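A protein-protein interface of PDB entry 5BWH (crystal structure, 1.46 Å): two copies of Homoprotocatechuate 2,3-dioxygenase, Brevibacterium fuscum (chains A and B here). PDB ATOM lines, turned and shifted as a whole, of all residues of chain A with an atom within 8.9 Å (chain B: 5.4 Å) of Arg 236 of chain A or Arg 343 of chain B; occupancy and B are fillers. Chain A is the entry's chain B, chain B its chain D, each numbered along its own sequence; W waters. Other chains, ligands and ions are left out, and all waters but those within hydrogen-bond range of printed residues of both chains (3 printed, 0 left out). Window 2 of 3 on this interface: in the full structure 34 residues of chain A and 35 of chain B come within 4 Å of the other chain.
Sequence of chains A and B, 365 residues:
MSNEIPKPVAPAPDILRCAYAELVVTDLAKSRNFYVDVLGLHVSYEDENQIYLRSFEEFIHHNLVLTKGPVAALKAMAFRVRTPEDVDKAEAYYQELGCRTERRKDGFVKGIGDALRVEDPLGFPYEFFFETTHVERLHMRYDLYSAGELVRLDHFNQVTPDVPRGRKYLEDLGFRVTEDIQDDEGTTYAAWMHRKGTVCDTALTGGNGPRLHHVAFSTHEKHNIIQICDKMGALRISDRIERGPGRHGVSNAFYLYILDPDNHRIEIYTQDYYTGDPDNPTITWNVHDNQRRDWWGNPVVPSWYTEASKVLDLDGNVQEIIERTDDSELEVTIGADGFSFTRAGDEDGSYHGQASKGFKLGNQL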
ATOM      1  N   VAL A  38      16.004 -15.606  -0.466  1.00  0.00           N
ATOM      2  CA  VAL A  38      14.850 -14.920  -1.000  1.00  0.00           C
ATOM      3  C   VAL A  38      15.074 -14.517  -2.447  1.00  0.00           C
ATOM      4  O   VAL A  38      14.300 -14.917  -3.316  1.00  0.00           O
ATOM      5  CB  VAL A  38      14.395 -13.722  -0.138  1.00  0.00           C
ATOM      6  CG1 VAL A  38      13.148 -13.087  -0.742  1.00  0.00           C
ATOM      7  CG2 VAL A  38      14.097 -14.185   1.286  1.00  0.00           C
ATOM      8  N   CYS A 229       7.303 -10.812  -5.634  1.00  0.00           N
ATOM      9  CA  CYS A 229       6.215 -10.406  -4.754  1.00  0.00           C
ATOM     10  C   CYS A 229       5.464 -11.628  -4.204  1.00  0.00           C
ATOM     11  O   CYS A 229       5.186 -11.711  -3.010  1.00  0.00           O
ATOM     12  CB  CYS A 229       5.208  -9.511  -5.501  1.00  0.00           C
ATOM     13  SG  CYS A 229       5.858  -7.973  -6.120  1.00  0.00           S
ATOM     14  N   ASP A 230       5.134 -12.548  -5.100  1.00  0.00           N
ATOM     15  CA  ASP A 230       4.409 -13.770  -4.711  1.00  0.00           C
ATOM     16  C   ASP A 230       5.198 -14.570  -3.679  1.00  0.00           C
ATOM     17  O   ASP A 230       4.636 -15.048  -2.683  1.00  0.00           O
ATOM     18  CB  ASP A 230       4.116 -14.644  -5.918  1.00  0.00           C
ATOM     19  CG  ASP A 230       3.066 -14.055  -6.857  1.00  0.00           C
ATOM     20  OD1 ASP A 230       2.181 -13.263  -6.426  1.00  0.00           O
ATOM     21  OD2 ASP A 230       3.094 -14.455  -8.043  1.00  0.00           O
ATOM     22  N   LYS A 231       6.504 -14.709  -3.913  1.00  0.00           N
ATOM     23  CA  LYS A 231       7.388 -15.410  -2.984  1.00  0.00           C
ATOM     24  C   LYS A 231       7.474 -14.707  -1.627  1.00  0.00           C
ATOM     25  O   LYS A 231       7.479 -15.361  -0.567  1.00  0.00           O
ATOM     26  CB  LYS A 231       8.795 -15.575  -3.581  1.00  0.00           C
ATOM     27  CG  LYS A 231       9.728 -16.402  -2.723  1.00  0.00           C
ATOM     28  CD  LYS A 231      11.065 -16.602  -3.412  1.00  0.00           C
ATOM     29  CE  LYS A 231      11.952 -17.528  -2.634  1.00  0.00           C
ATOM     30  NZ  LYS A 231      13.253 -17.712  -3.294  1.00  0.00           N
ATOM     31  N   MET A 232       7.555 -13.382  -1.638  1.00  0.00           N
ATOM     32  CA  MET A 232       7.564 -12.629  -0.384  1.00  0.00           C
ATOM     33  C   MET A 232       6.256 -12.797   0.406  1.00  0.00           C
ATOM     34  O   MET A 232       6.269 -12.925   1.630  1.00  0.00           O
ATOM     35  CB  MET A 232       7.937 -11.158  -0.637  1.00  0.00           C
ATOM     36  CG  MET A 232       9.377 -11.067  -1.122  1.00  0.00           C
ATOM     37  SD  MET A 232       9.926  -9.389  -1.470  1.00  0.00           S
ATOM     38  CE  MET A 232      10.078  -8.712   0.180  1.00  0.00           C
ATOM     39  N   GLY A 233       5.137 -12.887  -0.304  1.00  0.00           N
ATOM     40  CA  GLY A 233       3.895 -13.228   0.356  1.00  0.00           C
ATOM     41  C   GLY A 233       3.943 -14.621   0.964  1.00  0.00           C
ATOM     42  O   GLY A 233       3.527 -14.821   2.099  1.00  0.00           O
ATOM     43  N   ALA A 234       4.451 -15.599   0.221  1.00  0.00           N
ATOM     44  CA  ALA A 234       4.523 -16.968   0.737  1.00  0.00           C
ATOM     45  C   ALA A 234       5.436 -17.089   1.956  1.00  0.00           C
ATOM     46  O   ALA A 234       5.194 -17.906   2.846  1.00  0.00           O
ATOM     47  CB  ALA A 234       4.949 -17.907  -0.362  1.00  0.00           C
ATOM     48  N   LEU A 235       6.487 -16.271   1.979  1.00  0.00           N
ATOM     49  CA  LEU A 235       7.416 -16.254   3.085  1.00  0.00           C
ATOM     50  C   LEU A 235       6.922 -15.350   4.222  1.00  0.00           C
ATOM     51  O   LEU A 235       7.576 -15.247   5.268  1.00  0.00           O
ATOM     52  CB  LEU A 235       8.800 -15.776   2.617  1.00  0.00           C
ATOM     53  CG  LEU A 235       9.560 -16.747   1.705  1.00  0.00           C
ATOM     54  CD1 LEU A 235      10.833 -16.129   1.160  1.00  0.00           C
ATOM     55  CD2 LEU A 235       9.852 -18.043   2.439  1.00  0.00           C
ATOM     56  N   ARG A 236       5.758 -14.740   4.043  1.00  0.00           N
ATOM     57  CA  ARG A 236       5.121 -13.877   5.031  1.00  0.00           C
ATOM     58  C   ARG A 236       6.059 -12.720   5.416  1.00  0.00           C
ATOM     59  O   ARG A 236       6.168 -12.352   6.586  1.00  0.00           O
ATOM     60  CB  ARG A 236       4.612 -14.673   6.250  1.00  0.00           C
ATOM     61  CG  ARG A 236       3.344 -15.471   5.920  1.00  0.00           C
ATOM     62  CD  ARG A 236       2.143 -14.578   6.099  1.00  0.00           C
ATOM     63  NE  ARG A 236       0.903 -15.194   5.648  1.00  0.00           N
ATOM     64  CZ  ARG A 236      -0.284 -14.580   5.678  1.00  0.00           C
ATOM     65  NH1 ARG A 236      -0.408 -13.351   6.182  1.00  0.00           N
ATOM     66  NH2 ARG A 236      -1.353 -15.199   5.194  1.00  0.00           N
ATOM     67  N   ILE A 237       6.697 -12.150   4.388  1.00  0.00           N
ATOM     68  CA  ILE A 237       7.517 -10.950   4.513  1.00  0.00           C
ATOM     69  C   ILE A 237       7.057  -9.871   3.525  1.00  0.00           C
ATOM     70  O   ILE A 237       7.847  -9.039   3.058  1.00  0.00           O
ATOM     71  CB  ILE A 237       9.022 -11.255   4.340  1.00  0.00           C
ATOM     72  CG1 ILE A 237       9.345 -11.878   2.970  1.00  0.00           C
ATOM     73  CG2 ILE A 237       9.505 -12.154   5.470  1.00  0.00           C
ATOM     74  CD1 ILE A 237      10.808 -12.123   2.696  1.00  0.00           C
ATOM     75  N   SER A 238       5.752  -9.851   3.247  1.00  0.00           N
ATOM     76  CA  SER A 238       5.181  -8.811   2.403  1.00  0.00           C
ATOM     77  C   SER A 238       5.339  -7.407   2.955  1.00  0.00           C
ATOM     78  O   SER A 238       5.280  -6.445   2.201  1.00  0.00           O
ATOM     79  CB  SER A 238       3.701  -9.065   2.101  1.00  0.00           C
ATOM     80  OG  SER A 238       2.939  -9.080   3.270  1.00  0.00           O
ATOM     81  N   ASP A 239       5.536  -7.287   4.273  1.00  0.00           N
ATOM     82  CA  ASP A 239       5.884  -5.989   4.887  1.00  0.00           C
ATOM     83  C   ASP A 239       7.218  -5.432   4.418  1.00  0.00           C
ATOM     84  O   ASP A 239       7.469  -4.249   4.654  1.00  0.00           O
ATOM     85  CB  ASP A 239       5.855  -6.045   6.433  1.00  0.00           C
ATOM     86  CG  ASP A 239       6.764  -7.116   7.033  1.00  0.00           C
ATOM     87  OD1 ASP A 239       6.934  -8.214   6.435  1.00  0.00           O
ATOM     88  OD2 ASP A 239       7.278  -6.858   8.165  1.00  0.00           O
ATOM     89  N   ARG A 240       8.054  -6.268   3.774  1.00  0.00           N
ATOM     90  CA  ARG A 240       9.318  -5.815   3.206  1.00  0.00           C
ATOM     91  C   ARG A 240       9.183  -5.389   1.737  1.00  0.00           C
ATOM     92  O   ARG A 240      10.175  -4.973   1.112  1.00  0.00           O
ATOM     93  CB  ARG A 240      10.411  -6.877   3.414  1.00  0.00           C
ATOM     94  CG  ARG A 240      10.523  -7.374   4.851  1.00  0.00           C
ATOM     95  CD  ARG A 240      10.668  -6.252   5.861  1.00  0.00           C
ATOM     96  NE  ARG A 240      11.970  -5.602   5.747  1.00  0.00           N
ATOM     97  CZ  ARG A 240      12.297  -4.477   6.371  1.00  0.00           C
ATOM     98  NH1 ARG A 240      11.411  -3.828   7.096  1.00  0.00           N
ATOM     99  NH2 ARG A 240      13.513  -3.986   6.240  1.00  0.00           N
ATOM    100  N   ILE A 241       7.968  -5.483   1.189  1.00  0.00           N
ATOM    101  CA  ILE A 241       7.645  -4.863  -0.091  1.00  0.00           C
ATOM    102  C   ILE A 241       7.252  -3.429   0.211  1.00  0.00           C
ATOM    103  O   ILE A 241       6.233  -3.187   0.863  1.00  0.00           O
ATOM    104  CB  ILE A 241       6.485  -5.570  -0.850  1.00  0.00           C
ATOM    105  CG1 ILE A 241       6.844  -7.024  -1.168  1.00  0.00           C
ATOM    106  CG2 ILE A 241       6.127  -4.799  -2.118  1.00  0.00           C
ATOM    107  CD1 ILE A 241       5.691  -7.846  -1.672  1.00  0.00           C
ATOM    108  N   TRP B 285      -9.994 -17.140   5.750  1.00  0.00           N
ATOM    109  CA  TRP B 285      -9.016 -16.159   6.145  1.00  0.00           C
ATOM    110  C   TRP B 285      -9.526 -15.292   7.272  1.00  0.00           C
ATOM    111  O   TRP B 285     -10.712 -14.964   7.337  1.00  0.00           O
ATOM    112  CB  TRP B 285      -8.682 -15.257   4.966  1.00  0.00           C
ATOM    113  CG  TRP B 285      -8.155 -15.925   3.735  1.00  0.00           C
ATOM    114  CD1 TRP B 285      -8.860 -16.668   2.830  1.00  0.00           C
ATOM    115  CD2 TRP B 285      -6.817 -15.845   3.212  1.00  0.00           C
ATOM    116  NE1 TRP B 285      -8.045 -17.084   1.804  1.00  0.00           N
ATOM    117  CE2 TRP B 285      -6.788 -16.605   2.015  1.00  0.00           C
ATOM    118  CE3 TRP B 285      -5.638 -15.260   3.667  1.00  0.00           C
ATOM    119  CZ2 TRP B 285      -5.632 -16.760   1.243  1.00  0.00           C
ATOM    120  CZ3 TRP B 285      -4.498 -15.410   2.905  1.00  0.00           C
ATOM    121  CH2 TRP B 285      -4.508 -16.144   1.689  1.00  0.00           C
ATOM    122  N   ASP B 289      -5.841 -10.335   8.499  1.00  0.00           N
ATOM    123  CA  ASP B 289      -4.690 -10.805   7.726  1.00  0.00           C
ATOM    124  C   ASP B 289      -4.506  -9.879   6.512  1.00  0.00           C
ATOM    125  O   ASP B 289      -5.288  -9.900   5.560  1.00  0.00           O
ATOM    126  CB  ASP B 289      -4.898 -12.280   7.339  1.00  0.00           C
ATOM    127  CG  ASP B 289      -3.740 -12.891   6.589  1.00  0.00           C
ATOM    128  OD1 ASP B 289      -2.898 -12.156   6.028  1.00  0.00           O
ATOM    129  OD2 ASP B 289      -3.702 -14.138   6.556  1.00  0.00           O
ATOM    130  N   ASN B 290      -3.438  -9.096   6.538  1.00  0.00           N
ATOM    131  CA  ASN B 290      -3.173  -8.124   5.472  1.00  0.00           C
ATOM    132  C   ASN B 290      -2.760  -8.759   4.131  1.00  0.00           C
ATOM    133  O   ASN B 290      -2.541  -8.020   3.166  1.00  0.00           O
ATOM    134  CB  ASN B 290      -2.104  -7.111   5.901  1.00  0.00           C
ATOM    135  CG  ASN B 290      -2.021  -5.922   4.966  1.00  0.00           C
ATOM    136  OD1 ASN B 290      -3.032  -5.247   4.706  1.00  0.00           O
ATOM    137  ND2 ASN B 290      -0.817  -5.640   4.464  1.00  0.00           N
ATOM    138  N   GLN B 291      -2.634 -10.093   4.067  1.00  0.00           N
ATOM    139  CA  GLN B 291      -2.403 -10.776   2.774  1.00  0.00           C
ATOM    140  C   GLN B 291      -3.659 -11.453   2.211  1.00  0.00           C
ATOM    141  O   GLN B 291      -3.581 -12.113   1.183  1.00  0.00           O
ATOM    142  CB  GLN B 291      -1.258 -11.813   2.893  1.00  0.00           C
ATOM    143  CG  GLN B 291       0.103 -11.146   3.178  1.00  0.00           C
ATOM    144  CD  GLN B 291       1.327 -12.072   3.205  1.00  0.00           C
ATOM    145  OE1 GLN B 291       2.432 -11.635   3.567  1.00  0.00           O
ATOM    146  NE2 GLN B 291       1.157 -13.324   2.783  1.00  0.00           N
ATOM    147  N   TRP B 295      -2.286 -10.232  -1.671  1.00  0.00           N
ATOM    148  CA  TRP B 295      -1.295 -11.145  -1.120  1.00  0.00           C
ATOM    149  C   TRP B 295       0.030 -10.448  -0.800  1.00  0.00           C
ATOM    150  O   TRP B 295       0.781 -10.896   0.061  1.00  0.00           O
ATOM    151  CB  TRP B 295      -1.062 -12.224  -2.154  1.00  0.00           C
ATOM    152  CG  TRP B 295      -0.089 -13.322  -1.836  1.00  0.00           C
ATOM    153  CD1 TRP B 295       1.024 -13.635  -2.554  1.00  0.00           C
ATOM    154  CD2 TRP B 295      -0.174 -14.306  -0.794  1.00  0.00           C
ATOM    155  NE1 TRP B 295       1.653 -14.744  -2.015  1.00  0.00           N
ATOM    156  CE2 TRP B 295       0.927 -15.183  -0.951  1.00  0.00           C
ATOM    157  CE3 TRP B 295      -1.072 -14.551   0.246  1.00  0.00           C
ATOM    158  CZ2 TRP B 295       1.145 -16.266  -0.107  1.00  0.00           C
ATOM    159  CZ3 TRP B 295      -0.835 -15.607   1.090  1.00  0.00           C
ATOM    160  CH2 TRP B 295       0.247 -16.465   0.898  1.00  0.00           C
ATOM    161  N   PHE B 341      -2.371  -7.362  10.165  1.00  0.00           N
ATOM    162  CA  PHE B 341      -1.050  -7.948  10.413  1.00  0.00           C
ATOM    163  C   PHE B 341      -0.473  -8.587   9.158  1.00  0.00           C
ATOM    164  O   PHE B 341      -1.205  -8.976   8.238  1.00  0.00           O
ATOM    165  CB  PHE B 341      -1.106  -8.982  11.551  1.00  0.00           C
ATOM    166  CG  PHE B 341      -1.993 -10.185  11.281  1.00  0.00           C
ATOM    167  CD1 PHE B 341      -3.248 -10.286  11.871  1.00  0.00           C
ATOM    168  CD2 PHE B 341      -1.575 -11.226  10.425  1.00  0.00           C
ATOM    169  CE1 PHE B 341      -4.062 -11.396  11.634  1.00  0.00           C
ATOM    170  CE2 PHE B 341      -2.390 -12.323  10.186  1.00  0.00           C
ATOM    171  CZ  PHE B 341      -3.635 -12.410  10.801  1.00  0.00           C
ATOM    172  N   THR B 342       0.844  -8.727   9.140  1.00  0.00           N
ATOM    173  CA  THR B 342       1.529  -9.523   8.120  1.00  0.00           C
ATOM    174  C   THR B 342       1.700 -10.959   8.608  1.00  0.00           C
ATOM    175  O   THR B 342       1.426 -11.907   7.883  1.00  0.00           O
ATOM    176  CB  THR B 342       2.897  -8.908   7.783  1.00  0.00           C
ATOM    177  OG1 THR B 342       2.705  -7.564   7.320  1.00  0.00           O
ATOM    178  CG2 THR B 342       3.597  -9.695   6.721  1.00  0.00           C
ATOM    179  N   ARG B 343       2.150 -11.097   9.845  1.00  0.00           N
ATOM    180  CA  ARG B 343       2.306 -12.393  10.512  1.00  0.00           C
ATOM    181  C   ARG B 343       1.421 -12.354  11.745  1.00  0.00           C
ATOM    182  O   ARG B 343       1.529 -11.436  12.573  1.00  0.00           O
ATOM    183  CB  ARG B 343       3.763 -12.642  10.897  1.00  0.00           C
ATOM    184  CG  ARG B 343       4.721 -12.759   9.714  1.00  0.00           C
ATOM    185  CD  ARG B 343       6.170 -12.575  10.137  1.00  0.00           C
ATOM    186  NE  ARG B 343       6.431 -11.203  10.546  1.00  0.00           N
ATOM    187  CZ  ARG B 343       6.679 -10.189   9.722  1.00  0.00           C
ATOM    188  NH1 ARG B 343       6.787 -10.373   8.413  1.00  0.00           N
ATOM    189  NH2 ARG B 343       6.859  -8.976  10.224  1.00  0.00           N
ATOM    190  N   ALA B 344       0.542 -13.347  11.869  1.00  0.00           N
ATOM    191  CA  ALA B 344      -0.379 -13.385  13.004  1.00  0.00           C
ATOM    192  C   ALA B 344       0.415 -13.345  14.319  1.00  0.00           C
ATOM    193  O   ALA B 344       1.404 -14.066  14.491  1.00  0.00           O
ATOM    194  CB  ALA B 344      -1.284 -14.617  12.931  1.00  0.00           C
ATOM    195  N   GLY B 345       0.015 -12.451  15.216  1.00  0.00           N
ATOM    196  CA  GLY B 345       0.695 -12.315  16.497  1.00  0.00           C
ATOM    197  C   GLY B 345       1.925 -11.423  16.538  1.00  0.00           C
ATOM    198  O   GLY B 345       2.455 -11.172  17.614  1.00  0.00           O
ATOM    199  N   ASP B 346       2.388 -10.946  15.386  1.00  0.00           N
ATOM    200  CA  ASP B 346       3.605 -10.121  15.311  1.00  0.00           C
ATOM    201  C   ASP B 346       3.261  -8.630  15.154  1.00  0.00           C
ATOM    202  O   ASP B 346       2.549  -8.254  14.228  1.00  0.00           O
ATOM    203  CB  ASP B 346       4.438 -10.587  14.129  1.00  0.00           C
ATOM    204  CG  ASP B 346       5.845 -10.023  14.115  1.00  0.00           C
ATOM    205  OD1 ASP B 346       6.218  -9.208  14.978  1.00  0.00           O
ATOM    206  OD2 ASP B 346       6.596 -10.431  13.198  1.00  0.00           O
ATOM    207  N   ASP B 348       5.537  -6.381  14.493  1.00  0.00           N
ATOM    208  CA  ASP B 348       6.330  -5.971  13.321  1.00  0.00           C
ATOM    209  C   ASP B 348       5.542  -6.322  12.072  1.00  0.00           C
ATOM    210  O   ASP B 348       5.117  -7.465  11.918  1.00  0.00           O
ATOM    211  CB  ASP B 348       7.673  -6.697  13.260  1.00  0.00           C
ATOM    212  CG  ASP B 348       8.584  -6.361  14.413  1.00  0.00           C
ATOM    213  OD1 ASP B 348       8.499  -5.245  14.966  1.00  0.00           O
ATOM    214  OD2 ASP B 348       9.389  -7.234  14.773  1.00  0.00           O
ATOM    215  N   GLY B 349       5.366  -5.346  11.188  1.00  0.00           N
ATOM    216  CA  GLY B 349       4.584  -5.516   9.978  1.00  0.00           C
ATOM    217  C   GLY B 349       3.089  -5.507  10.233  1.00  0.00           C
ATOM    218  O   GLY B 349       2.291  -5.957   9.375  1.00  0.00           O
HETATM  219  O   HOH W   1       9.690  -8.796   8.184  1.00  0.00           O
HETATM  220  O   HOH W   2      -2.285 -15.611   8.531  1.00  0.00           O
HETATM  221  O   HOH W   3       1.707  -7.154   4.746  1.00  0.00           O
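The side-chain carboxylate (OD1) of Asp 289 of chain B lies within hydrogen-bond range of the backbone NH (N) of Gln 291 of chain B (2.9 Å).
The side-chain hydroxyl of Thr 342 of chain B sits at hydrogen-bond distance from the backbone carbonyl oxygen of Gly 349 of chain B (2.6 Å).
The guanidinium group (NE) of Arg 343 of chain B lies within salt-bridge range of the side-chain carboxylate (OD2) of Asp 346 of chain B, at 2.8 Å.
O of Asp 348 of chain B is in hydrogen-bond range of NH2 of Arg 343 of chain B, at 2.9 Å.
No position is printed for both chains.
Of the 14 pairs that touch across the chains among the printed residues, none has its exchanged pair printed and touching as well.
The indole nitrogen of Trp 295 of chain B is in hydrogen-bond range of the backbone carbonyl oxygen of Asp 230 of chain A (3.1 Å).
The side-chain amide nitrogen (NE2) of Gln 291 of chain B is in hydrogen-bond range of the backbone carbonyl oxygen (O) of Gly 233 of chain A (2.9 Å).
NH1 of Arg 236 of chain A is in salt-bridge range of OD1 of Asp 289 of chain B (2.8 Å).
The side-chain amide nitrogen (NE2) of Gln 291 of chain B sits close to the guanidinium group (NE) of Arg 236 of chain A (3.4 Å).
NH1 of Arg 236 of chain A is in hydrogen-bond range of O of Thr 342 of chain B, 2.9 Å away.
The backbone carbonyl oxygen (O) of Arg 236 of chain A sits at hydrogen-bond distance from the guanidinium group (NH1) of Arg 343 of chain B, at 2.8 Å.
OE1 of Gln 291 of chain B lies within hydrogen-bond range of OG of Ser 238 of chain A (2.6 Å).
NH1 of Arg 343 of chain B lies within salt-bridge range of OD1 of Asp 239 of chain A (2.9 Å).
Of the 14 printed residues of chain A, 6 touch a printed residue of chain B.
Hydrophobic or aromatic side chains of chain B that line the printed part of chain A: Trp 285 and Trp 295.
Among the printed residues, 14 pairs touch across the chains.
Water W3 lies within hydrogen-bond range of the side-chain hydroxyl (OG) of Ser 238 of chain A (2.7 Å), the side-chain hydroxyl (OG1) of Thr 342 of chain B (2.8 Å) and the side-chain amide nitrogen (ND2) of Asn 290 of chain B (3.0 Å).
Water W2 lies within hydrogen-bond range of the side-chain carboxylate of Asp 289 of chain B and the guanidinium group of Arg 236 of chain A.
Water W1 lies within hydrogen-bond range of OD2 of Asp 239 of chain A and NH1 of Arg 343 of chain B.
CZ2 of Trp 295 of chain B touches C of Gly 233 of chain A (3.4 Å).
Ala 234 of chain A touches Trp 295 of chain B.
NH2 of Arg 236 of chain A touches CZ3 of Trp 285 of chain B (3.9 Å).
CG2 of Thr 342 of chain B touches OG of Ser 238 of chain A, at 3.6 Å.
OG1 of Thr 342 of chain B touches CB of Asp 239 of chain A (3.6 Å).
CA of Gly 349 of chain B touches OD2 of Asp 239 of chain A (3.5 Å).
Of chain B, only Trp 285, Asp 289, Gln 291, Thr 342 and Arg 343 come within 4 Å of Arg 236 of chain A.
Of the printed residues of chain A, Arg 343 of chain B touches Arg 236 and Asp 239.
Thr 342 of chain B touches just these residues of chain A: Arg 236, Ser 238 and Asp 239.
Ala 344 of chain B touches none of the printed residues of chain A.
No residue of chain A comes within 4 Å of Asp 346 of chain B.
Of the printed residues of chain B, Asp 230 of chain A touches Trp 295.
Printed residues of chain B within 4 Å of Asp 239 of chain A: Thr 342 (3.6 Å), Arg 343 (2.9 Å) and Gly 349 (3.5 Å).
Printed residues of chain B within 4 Å of Gly 233 of chain A: Gln 291 and Trp 295.
Ile 237 of chain A touches none of the printed residues of chain B.
The nearest residue of chain B that does not touch Arg 236 of chain A is Trp 295 of chain B (4.2 Å).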
